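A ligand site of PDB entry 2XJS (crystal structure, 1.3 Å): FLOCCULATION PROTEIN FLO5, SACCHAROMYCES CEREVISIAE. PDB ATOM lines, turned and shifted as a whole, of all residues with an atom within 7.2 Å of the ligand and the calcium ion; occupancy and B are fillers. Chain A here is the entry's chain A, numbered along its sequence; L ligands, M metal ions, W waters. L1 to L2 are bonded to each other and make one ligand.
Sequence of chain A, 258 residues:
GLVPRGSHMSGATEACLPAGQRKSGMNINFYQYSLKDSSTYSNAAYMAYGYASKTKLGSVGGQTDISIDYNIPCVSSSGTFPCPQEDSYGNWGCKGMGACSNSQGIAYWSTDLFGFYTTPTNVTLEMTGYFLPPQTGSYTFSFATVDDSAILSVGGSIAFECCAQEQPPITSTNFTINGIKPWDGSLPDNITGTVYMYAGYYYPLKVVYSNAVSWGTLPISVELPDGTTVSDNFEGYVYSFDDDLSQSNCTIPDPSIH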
ATOM      1  N   LYS A  36      -1.947   4.535   3.662  1.00  0.00           N
ATOM      2  CA  LYS A  36      -1.915   5.465   2.511  1.00  0.00           C
ATOM      3  C   LYS A  36      -0.637   6.287   2.373  1.00  0.00           C
ATOM      4  O   LYS A  36      -0.606   7.251   1.620  1.00  0.00           O
ATOM      5  CB  LYS A  36      -3.202   6.290   2.423  1.00  0.00           C
ATOM      6  CG  LYS A  36      -4.423   5.432   2.083  1.00  0.00           C
ATOM      7  CD  LYS A  36      -5.796   6.080   2.091  1.00  0.00           C
ATOM      8  CE  LYS A  36      -6.146   6.492   3.506  1.00  0.00           C
ATOM      9  NZ  LYS A  36      -7.541   6.933   3.669  1.00  0.00           N
ATOM     10  N   SER A  38       2.299   6.599   0.516  1.00  0.00           N
ATOM     11  CA  SER A  38       2.796   6.099  -0.761  1.00  0.00           C
ATOM     12  C   SER A  38       4.214   6.539  -1.099  1.00  0.00           C
ATOM     13  O   SER A  38       4.608   6.372  -2.270  1.00  0.00           O
ATOM     14  CB  SER A  38       1.874   6.579  -1.893  1.00  0.00           C
ATOM     15  OG  SER A  38       1.669   7.975  -1.886  1.00  0.00           O
ATOM     16  N   TYR A  41       7.966   3.679   1.426  1.00  0.00           N
ATOM     17  CA  TYR A  41       8.382   2.405   0.851  1.00  0.00           C
ATOM     18  C   TYR A  41       9.069   2.466  -0.502  1.00  0.00           C
ATOM     19  O   TYR A  41       9.382   1.433  -1.082  1.00  0.00           O
ATOM     20  CB  TYR A  41       7.168   1.458   0.824  1.00  0.00           C
ATOM     21  CG  TYR A  41       5.959   1.819  -0.012  1.00  0.00           C
ATOM     22  CD1 TYR A  41       4.719   1.274   0.284  1.00  0.00           C
ATOM     23  CD2 TYR A  41       5.983   2.721  -1.073  1.00  0.00           C
ATOM     24  CE1 TYR A  41       3.583   1.585  -0.459  1.00  0.00           C
ATOM     25  CE2 TYR A  41       4.856   3.061  -1.816  1.00  0.00           C
ATOM     26  CZ  TYR A  41       3.634   2.468  -1.515  1.00  0.00           C
ATOM     27  OH  TYR A  41       2.492   2.764  -2.239  1.00  0.00           O
ATOM     28  N   TYR A  70      -3.348 -11.056   0.295  1.00  0.00           N
ATOM     29  CA  TYR A  70      -4.291 -10.422   1.219  1.00  0.00           C
ATOM     30  C   TYR A  70      -5.356  -9.711   0.395  1.00  0.00           C
ATOM     31  O   TYR A  70      -5.050  -8.831  -0.436  1.00  0.00           O
ATOM     32  CB  TYR A  70      -3.569  -9.389   2.111  1.00  0.00           C
ATOM     33  CG  TYR A  70      -4.594  -8.618   2.923  1.00  0.00           C
ATOM     34  CD1 TYR A  70      -5.386  -9.226   3.880  1.00  0.00           C
ATOM     35  CD2 TYR A  70      -4.813  -7.278   2.635  1.00  0.00           C
ATOM     36  CE1 TYR A  70      -6.410  -8.524   4.563  1.00  0.00           C
ATOM     37  CE2 TYR A  70      -5.803  -6.591   3.318  1.00  0.00           C
ATOM     38  CZ  TYR A  70      -6.596  -7.187   4.261  1.00  0.00           C
ATOM     39  OH  TYR A  70      -7.581  -6.474   4.890  1.00  0.00           O
ATOM     40  N   ILE A  72      -9.013  -7.496   0.887  1.00  0.00           N
ATOM     41  CA  ILE A  72      -9.849  -6.754   1.790  1.00  0.00           C
ATOM     42  C   ILE A  72     -11.274  -7.326   1.861  1.00  0.00           C
ATOM     43  O   ILE A  72     -11.741  -7.980   0.913  1.00  0.00           O
ATOM     44  CB  ILE A  72      -9.911  -5.242   1.476  1.00  0.00           C
ATOM     45  CG1 ILE A  72     -10.416  -4.936   0.067  1.00  0.00           C
ATOM     46  CG2 ILE A  72      -8.556  -4.536   1.763  1.00  0.00           C
ATOM     47  CD1 ILE A  72     -10.903  -3.508  -0.168  1.00  0.00           C
ATOM     48  N   GLN A  85      -9.041  -9.107  -5.784  1.00  0.00           N
ATOM     49  CA  GLN A  85      -9.001  -7.779  -6.388  1.00  0.00           C
ATOM     50  C   GLN A  85      -9.581  -7.782  -7.807  1.00  0.00           C
ATOM     51  O   GLN A  85     -10.230  -6.830  -8.227  1.00  0.00           O
ATOM     52  CB  GLN A  85      -7.581  -7.233  -6.383  1.00  0.00           C
ATOM     53  CG  GLN A  85      -7.489  -5.746  -6.770  1.00  0.00           C
ATOM     54  CD  GLN A  85      -6.143  -5.047  -6.568  1.00  0.00           C
ATOM     55  OE1 GLN A  85      -6.102  -3.810  -6.697  1.00  0.00           O
ATOM     56  NE2 GLN A  85      -5.059  -5.782  -6.299  1.00  0.00           N
ATOM     57  N   SER A 103     -15.511   0.923   3.056  1.00  0.00           N
ATOM     58  CA  SER A 103     -14.501   1.670   2.314  1.00  0.00           C
ATOM     59  C   SER A 103     -13.276   0.865   1.951  1.00  0.00           C
ATOM     60  O   SER A 103     -12.746   0.122   2.765  1.00  0.00           O
ATOM     61  CB  SER A 103     -14.039   2.864   3.145  1.00  0.00           C
ATOM     62  OG  SER A 103     -13.020   3.626   2.497  1.00  0.00           O
ATOM     63  N   GLN A 104     -12.760   1.012   0.744  1.00  0.00           N
ATOM     64  CA  GLN A 104     -11.461   0.470   0.368  1.00  0.00           C
ATOM     65  C   GLN A 104     -10.299   1.225   0.988  1.00  0.00           C
ATOM     66  O   GLN A 104      -9.142   0.786   0.864  1.00  0.00           O
ATOM     67  CB  GLN A 104     -11.286   0.464  -1.142  1.00  0.00           C
ATOM     68  CG  GLN A 104     -12.212  -0.374  -1.948  1.00  0.00           C
ATOM     69  CD  GLN A 104     -11.815  -0.505  -3.423  1.00  0.00           C
ATOM     70  OE1 GLN A 104     -10.709  -0.142  -3.814  1.00  0.00           O
ATOM     71  NE2 GLN A 104     -12.689  -1.094  -4.228  1.00  0.00           N
ATOM     72  N   GLY A 105     -10.541   2.369   1.620  1.00  0.00           N
ATOM     73  CA  GLY A 105      -9.500   3.274   2.074  1.00  0.00           C
ATOM     74  C   GLY A 105      -9.202   3.311   3.555  1.00  0.00           C
ATOM     75  O   GLY A 105      -8.487   4.223   3.973  1.00  0.00           O
ATOM     76  N   ILE A 106      -9.769   2.417   4.350  1.00  0.00           N
ATOM     77  CA  ILE A 106      -9.523   2.319   5.788  1.00  0.00           C
ATOM     78  C   ILE A 106      -8.611   1.149   6.090  1.00  0.00           C
ATOM     79  O   ILE A 106      -8.427   0.249   5.251  1.00  0.00           O
ATOM     80  CB  ILE A 106     -10.830   2.291   6.598  1.00  0.00           C
ATOM     81  CG1 ILE A 106     -11.682   1.033   6.332  1.00  0.00           C
ATOM     82  CG2 ILE A 106     -11.673   3.605   6.418  1.00  0.00           C
ATOM     83  CD1 ILE A 106     -12.857   0.908   7.290  1.00  0.00           C
ATOM     84  N   PRO A 120      -3.188  -5.876   7.648  1.00  0.00           N
ATOM     85  CA  PRO A 120      -2.485  -6.222   6.407  1.00  0.00           C
ATOM     86  C   PRO A 120      -2.555  -5.131   5.350  1.00  0.00           C
ATOM     87  O   PRO A 120      -1.789  -5.174   4.396  1.00  0.00           O
ATOM     88  CB  PRO A 120      -3.112  -7.546   5.955  1.00  0.00           C
ATOM     89  CG  PRO A 120      -3.601  -8.105   7.202  1.00  0.00           C
ATOM     90  CD  PRO A 120      -4.173  -6.921   7.995  1.00  0.00           C
ATOM     91  N   THR A 121      -3.529  -4.240   5.476  1.00  0.00           N
ATOM     92  CA  THR A 121      -3.655  -3.054   4.634  1.00  0.00           C
ATOM     93  C   THR A 121      -2.476  -2.116   4.702  1.00  0.00           C
ATOM     94  O   THR A 121      -2.267  -1.349   3.774  1.00  0.00           O
ATOM     95  CB  THR A 121      -4.931  -2.256   5.034  1.00  0.00           C
ATOM     96  OG1 THR A 121      -4.949  -2.114   6.459  1.00  0.00           O
ATOM     97  CG2 THR A 121      -6.211  -2.952   4.621  1.00  0.00           C
ATOM     98  N   ASP A 147       2.558  -5.802  -4.754  1.00  0.00           N
ATOM     99  CA  ASP A 147       1.609  -4.802  -4.307  1.00  0.00           C
ATOM    100  C   ASP A 147       1.791  -4.706  -2.790  1.00  0.00           C
ATOM    101  O   ASP A 147       1.314  -5.606  -2.090  1.00  0.00           O
ATOM    102  CB  ASP A 147       0.183  -5.156  -4.721  1.00  0.00           C
ATOM    103  CG  ASP A 147      -0.894  -4.173  -4.246  1.00  0.00           C
ATOM    104  OD1 ASP A 147      -2.045  -4.194  -4.748  1.00  0.00           O
ATOM    105  OD2 ASP A 147      -0.653  -3.372  -3.336  1.00  0.00           O
ATOM    106  N   ASP A 148       2.480  -3.681  -2.264  1.00  0.00           N
ATOM    107  CA  ASP A 148       2.973  -2.460  -2.932  1.00  0.00           C
ATOM    108  C   ASP A 148       4.479  -2.420  -3.227  1.00  0.00           C
ATOM    109  O   ASP A 148       4.828  -1.907  -4.297  1.00  0.00           O
ATOM    110  CB  ASP A 148       2.611  -1.235  -2.076  1.00  0.00           C
ATOM    111  CG  ASP A 148       1.155  -0.843  -2.233  1.00  0.00           C
ATOM    112  OD1 ASP A 148       0.740  -0.380  -3.341  1.00  0.00           O
ATOM    113  OD2 ASP A 148       0.374  -1.005  -1.263  1.00  0.00           O
ATOM    114  N   LYS A 181       8.640   0.071  -5.002  1.00  0.00           N
ATOM    115  CA  LYS A 181       7.644   0.845  -5.761  1.00  0.00           C
ATOM    116  C   LYS A 181       8.312   2.098  -6.324  1.00  0.00           C
ATOM    117  O   LYS A 181       8.827   2.895  -5.548  1.00  0.00           O
ATOM    118  CB  LYS A 181       6.465   1.215  -4.853  1.00  0.00           C
ATOM    119  CG  LYS A 181       5.288   1.837  -5.625  1.00  0.00           C
ATOM    120  CD  LYS A 181       4.367   0.724  -6.079  1.00  0.00           C
ATOM    121  CE  LYS A 181       3.522   0.972  -7.286  1.00  0.00           C
ATOM    122  NZ  LYS A 181       3.230  -0.331  -7.985  1.00  0.00           N
ATOM    123  N   TYR A 209       8.713  -6.671   2.672  1.00  0.00           N
ATOM    124  CA  TYR A 209       7.457  -6.429   1.968  1.00  0.00           C
ATOM    125  C   TYR A 209       6.640  -5.353   2.662  1.00  0.00           C
ATOM    126  O   TYR A 209       6.541  -5.362   3.871  1.00  0.00           O
ATOM    127  CB  TYR A 209       6.636  -7.761   1.966  1.00  0.00           C
ATOM    128  CG  TYR A 209       5.194  -7.499   1.555  1.00  0.00           C
ATOM    129  CD1 TYR A 209       4.861  -7.302   0.198  1.00  0.00           C
ATOM    130  CD2 TYR A 209       4.194  -7.303   2.484  1.00  0.00           C
ATOM    131  CE1 TYR A 209       3.599  -6.948  -0.172  1.00  0.00           C
ATOM    132  CE2 TYR A 209       2.910  -6.938   2.110  1.00  0.00           C
ATOM    133  CZ  TYR A 209       2.593  -6.767   0.775  1.00  0.00           C
ATOM    134  OH  TYR A 209       1.318  -6.408   0.454  1.00  0.00           O
ATOM    135  N   SER A 210       6.070  -4.425   1.874  1.00  0.00           N
ATOM    136  CA  SER A 210       5.215  -3.394   2.439  1.00  0.00           C
ATOM    137  C   SER A 210       3.911  -3.250   1.647  1.00  0.00           C
ATOM    138  O   SER A 210       3.886  -3.347   0.409  1.00  0.00           O
ATOM    139  CB  SER A 210       6.004  -2.092   2.553  1.00  0.00           C
ATOM    140  OG  SER A 210       5.325  -1.109   3.300  1.00  0.00           O
ATOM    141  N   ASN A 211       2.845  -2.999   2.389  1.00  0.00           N
ATOM    142  CA  ASN A 211       1.536  -2.615   1.863  1.00  0.00           C
ATOM    143  C   ASN A 211       1.144  -1.292   2.504  1.00  0.00           C
ATOM    144  O   ASN A 211       1.324  -1.151   3.716  1.00  0.00           O
ATOM    145  CB  ASN A 211       0.478  -3.679   2.157  1.00  0.00           C
ATOM    146  CG  ASN A 211      -0.777  -3.495   1.332  1.00  0.00           C
ATOM    147  OD1 ASN A 211      -0.766  -2.808   0.323  1.00  0.00           O
ATOM    148  ND2 ASN A 211      -1.847  -4.149   1.761  1.00  0.00           N
ATOM    149  N   ALA A 212       0.627  -0.357   1.701  1.00  0.00           N
ATOM    150  CA  ALA A 212       0.138   0.922   2.183  1.00  0.00           C
ATOM    151  C   ALA A 212      -1.373   1.051   2.221  1.00  0.00           C
ATOM    152  O   ALA A 212      -1.934   1.848   2.986  1.00  0.00           O
ATOM    153  CB  ALA A 212       0.643   2.091   1.332  1.00  0.00           C
ATOM    154  N   VAL A 213      -2.087   0.300   1.376  1.00  0.00           N
ATOM    155  CA  VAL A 213      -3.534   0.386   1.351  1.00  0.00           C
ATOM    156  C   VAL A 213      -4.082  -0.892   0.705  1.00  0.00           C
ATOM    157  O   VAL A 213      -3.471  -1.522  -0.161  1.00  0.00           O
ATOM    158  CB  VAL A 213      -4.017   1.642   0.652  1.00  0.00           C
ATOM    159  CG1 VAL A 213      -3.754   1.573  -0.836  1.00  0.00           C
ATOM    160  CG2 VAL A 213      -5.467   2.004   0.951  1.00  0.00           C
ATOM    161  N   SER A 214      -5.307  -1.209   1.115  1.00  0.00           N
ATOM    162  CA  SER A 214      -6.122  -2.283   0.569  1.00  0.00           C
ATOM    163  C   SER A 214      -5.331  -3.570   0.258  1.00  0.00           C
ATOM    164  O   SER A 214      -4.758  -4.150   1.190  1.00  0.00           O
ATOM    165  CB  SER A 214      -7.030  -1.783  -0.563  1.00  0.00           C
ATOM    166  OG  SER A 214      -6.291  -1.368  -1.705  1.00  0.00           O
ATOM    167  N   TRP A 215      -5.407  -4.079  -0.962  1.00  0.00           N
ATOM    168  CA  TRP A 215      -4.874  -5.401  -1.283  1.00  0.00           C
ATOM    169  C   TRP A 215      -3.368  -5.487  -1.116  1.00  0.00           C
ATOM    170  O   TRP A 215      -2.667  -4.491  -1.288  1.00  0.00           O
ATOM    171  CB  TRP A 215      -5.260  -5.777  -2.736  1.00  0.00           C
ATOM    172  CG  TRP A 215      -6.705  -6.107  -2.900  1.00  0.00           C
ATOM    173  CD1 TRP A 215      -7.246  -7.345  -2.781  1.00  0.00           C
ATOM    174  CD2 TRP A 215      -7.812  -5.234  -3.206  1.00  0.00           C
ATOM    175  NE1 TRP A 215      -8.591  -7.316  -2.972  1.00  0.00           N
ATOM    176  CE2 TRP A 215      -8.965  -6.030  -3.266  1.00  0.00           C
ATOM    177  CE3 TRP A 215      -7.914  -3.872  -3.473  1.00  0.00           C
ATOM    178  CZ2 TRP A 215     -10.227  -5.503  -3.535  1.00  0.00           C
ATOM    179  CZ3 TRP A 215      -9.198  -3.346  -3.777  1.00  0.00           C
ATOM    180  CH2 TRP A 215     -10.316  -4.191  -3.806  1.00  0.00           C
ATOM    181  N   GLY A 216      -2.909  -6.676  -0.761  1.00  0.00           N
ATOM    182  CA  GLY A 216      -1.474  -6.954  -0.659  1.00  0.00           C
ATOM    183  C   GLY A 216      -1.137  -8.204  -1.407  1.00  0.00           C
ATOM    184  O   GLY A 216      -1.811  -9.219  -1.186  1.00  0.00           O
ATOM    185  N   THR A 217      -0.096  -8.192  -2.240  1.00  0.00           N
ATOM    186  CA  THR A 217       0.190  -9.356  -3.078  1.00  0.00           C
ATOM    187  C   THR A 217       1.711  -9.481  -3.291  1.00  0.00           C
ATOM    188  O   THR A 217       2.392  -8.520  -3.682  1.00  0.00           O
ATOM    189  CB  THR A 217      -0.505  -9.230  -4.456  1.00  0.00           C
ATOM    190  OG1 THR A 217      -1.859  -8.789  -4.289  1.00  0.00           O
ATOM    191  CG2 THR A 217      -0.569 -10.598  -5.139  1.00  0.00           C
HETATM  192  C1  LIG L   1      -6.578   3.015  -5.064  1.00  0.00           C
HETATM  193  C2  LIG L   1      -7.039   1.604  -4.654  1.00  0.00           C
HETATM  194  C3  LIG L   1      -7.923   1.613  -3.389  1.00  0.00           C
HETATM  195  C4  LIG L   1      -7.305   2.493  -2.297  1.00  0.00           C
HETATM  196  C5  LIG L   1      -6.913   3.876  -2.826  1.00  0.00           C
HETATM  197  C6  LIG L   1      -6.257   4.743  -1.771  1.00  0.00           C
HETATM  198  O1  LIG L   1      -7.719   3.589  -5.670  1.00  0.00           O
HETATM  199  O2  LIG L   1      -5.887   0.816  -4.300  1.00  0.00           O
HETATM  200  O3  LIG L   1      -8.173   0.313  -2.911  1.00  0.00           O
HETATM  201  O4  LIG L   1      -8.231   2.698  -1.257  1.00  0.00           O
HETATM  202  O5  LIG L   1      -6.015   3.689  -3.938  1.00  0.00           O
HETATM  203  O6  LIG L   1      -6.095   6.062  -2.247  1.00  0.00           O
HETATM  204  C1  LG2 L   2      -5.202   0.194  -5.404  1.00  0.00           C
HETATM  205  C2  LG2 L   2      -4.908  -1.253  -4.987  1.00  0.00           C
HETATM  206  C3  LG2 L   2      -3.943  -1.201  -3.811  1.00  0.00           C
HETATM  207  C4  LG2 L   2      -2.680  -0.411  -4.115  1.00  0.00           C
HETATM  208  C5  LG2 L   2      -3.110   0.992  -4.561  1.00  0.00           C
HETATM  209  C6  LG2 L   2      -1.939   1.856  -4.989  1.00  0.00           C
HETATM  210  O1  LG2 L   2      -4.297  -1.953  -6.049  1.00  0.00           O
HETATM  211  O2  LG2 L   2      -3.675  -2.466  -3.306  1.00  0.00           O
HETATM  212  O3  LG2 L   2      -1.851  -0.356  -2.969  1.00  0.00           O
HETATM  213  O4  LG2 L   2      -4.008   0.897  -5.665  1.00  0.00           O
HETATM  214  O5  LG2 L   2      -1.298   1.266  -6.093  1.00  0.00           O
HETATM  215 CA    CA M   1      -1.847  -2.352  -1.701  1.00  0.00          CA
HETATM  216  O   HOH W   1     -10.291   4.648  -1.247  1.00  0.00           O
HETATM  217  O   HOH W   2      -4.321   7.763  -1.002  1.00  0.00           O
HETATM  218  O   HOH W   3      -3.354   3.307  -8.038  1.00  0.00           O
HETATM  219  O   HOH W   4       1.282   1.191  -5.149  1.00  0.00           O
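The calcium ion is bound by OD2 of Asp 147 (2.3 Å), O of Trp 215 (2.3 Å), OD1 of Asn 211 (2.3 Å), O3 of LG2 L2 (2.4 Å), O of Val 213 (2.4 Å), O2 of LG2 L2 (2.4 Å) and OD2 of Asp 148 (2.6 Å).
Water W4 lies within hydrogen-bond range of the side-chain carboxylate of Asp 148 and an oxygen (O5) of LG2 L2.
Five residues have an atom within 4 Å of the calcium ion: Asp 147, Asp 148, Asn 211, Val 213 and Trp 215. The nearest printed residue that does not touch the calcium ion is Ser 214 (4.2 Å).
O of Gly 105 is in hydrogen-bond range of NZ of Lys 36 (2.9 Å). The backbone NH (N) of Ala 212 sits close to the side-chain carboxylate (OD2) of Asp 148. The side-chain amide nitrogen (ND2) of Asn 211 is in hydrogen-bond range of the backbone carbonyl oxygen (O) of Pro 120 (2.8 Å). O of Ser 214 lies within hydrogen-bond range of ND2 of Asn 211 (3.0 Å). The backbone NH of Asp 148 sits at hydrogen-bond distance from the backbone carbonyl oxygen of Ser 210, 3.0 Å away. The backbone carbonyl oxygen (O) of Thr 121 sits at hydrogen-bond distance from the backbone NH (N) of Val 213 (2.9 Å). O of Asp 147 is in hydrogen-bond range of OH of Tyr 209 (2.7 Å). The backbone NH (N) of Asp 147 lies within hydrogen-bond range of the backbone carbonyl oxygen (O) of Thr 217, 2.9 Å away.
Gly 105 touches the ligand. Hydrophobic or aromatic side chains that line the ligand: Val 213 and Trp 215. Within 4 Å of the ligand: Gln 85, Gln 104, Gly 105, Asp 147, Asp 148, Val 213, Ser 214 and Trp 215. The nearest printed residue that does not touch the ligand is Lys 36 (4.1 Å).
The backbone NH of Trp 215 sits close to an oxygen (O2) of LG2 L2. An oxygen (O3) of LIG L1 is in hydrogen-bond range of the side-chain hydroxyl (OG) of Ser 214, at 2.8 Å. O of Gln 104 lies within hydrogen-bond range of O4 of LIG L1 (3.0 Å). The side-chain amide oxygen of Gln 104 is in hydrogen-bond range of an oxygen (O3) of LIG L1, at 2.7 Å. The side-chain amide oxygen (OE1) of Gln 85 is in hydrogen-bond range of an oxygen (O1) of LG2 L2 (2.7 Å).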
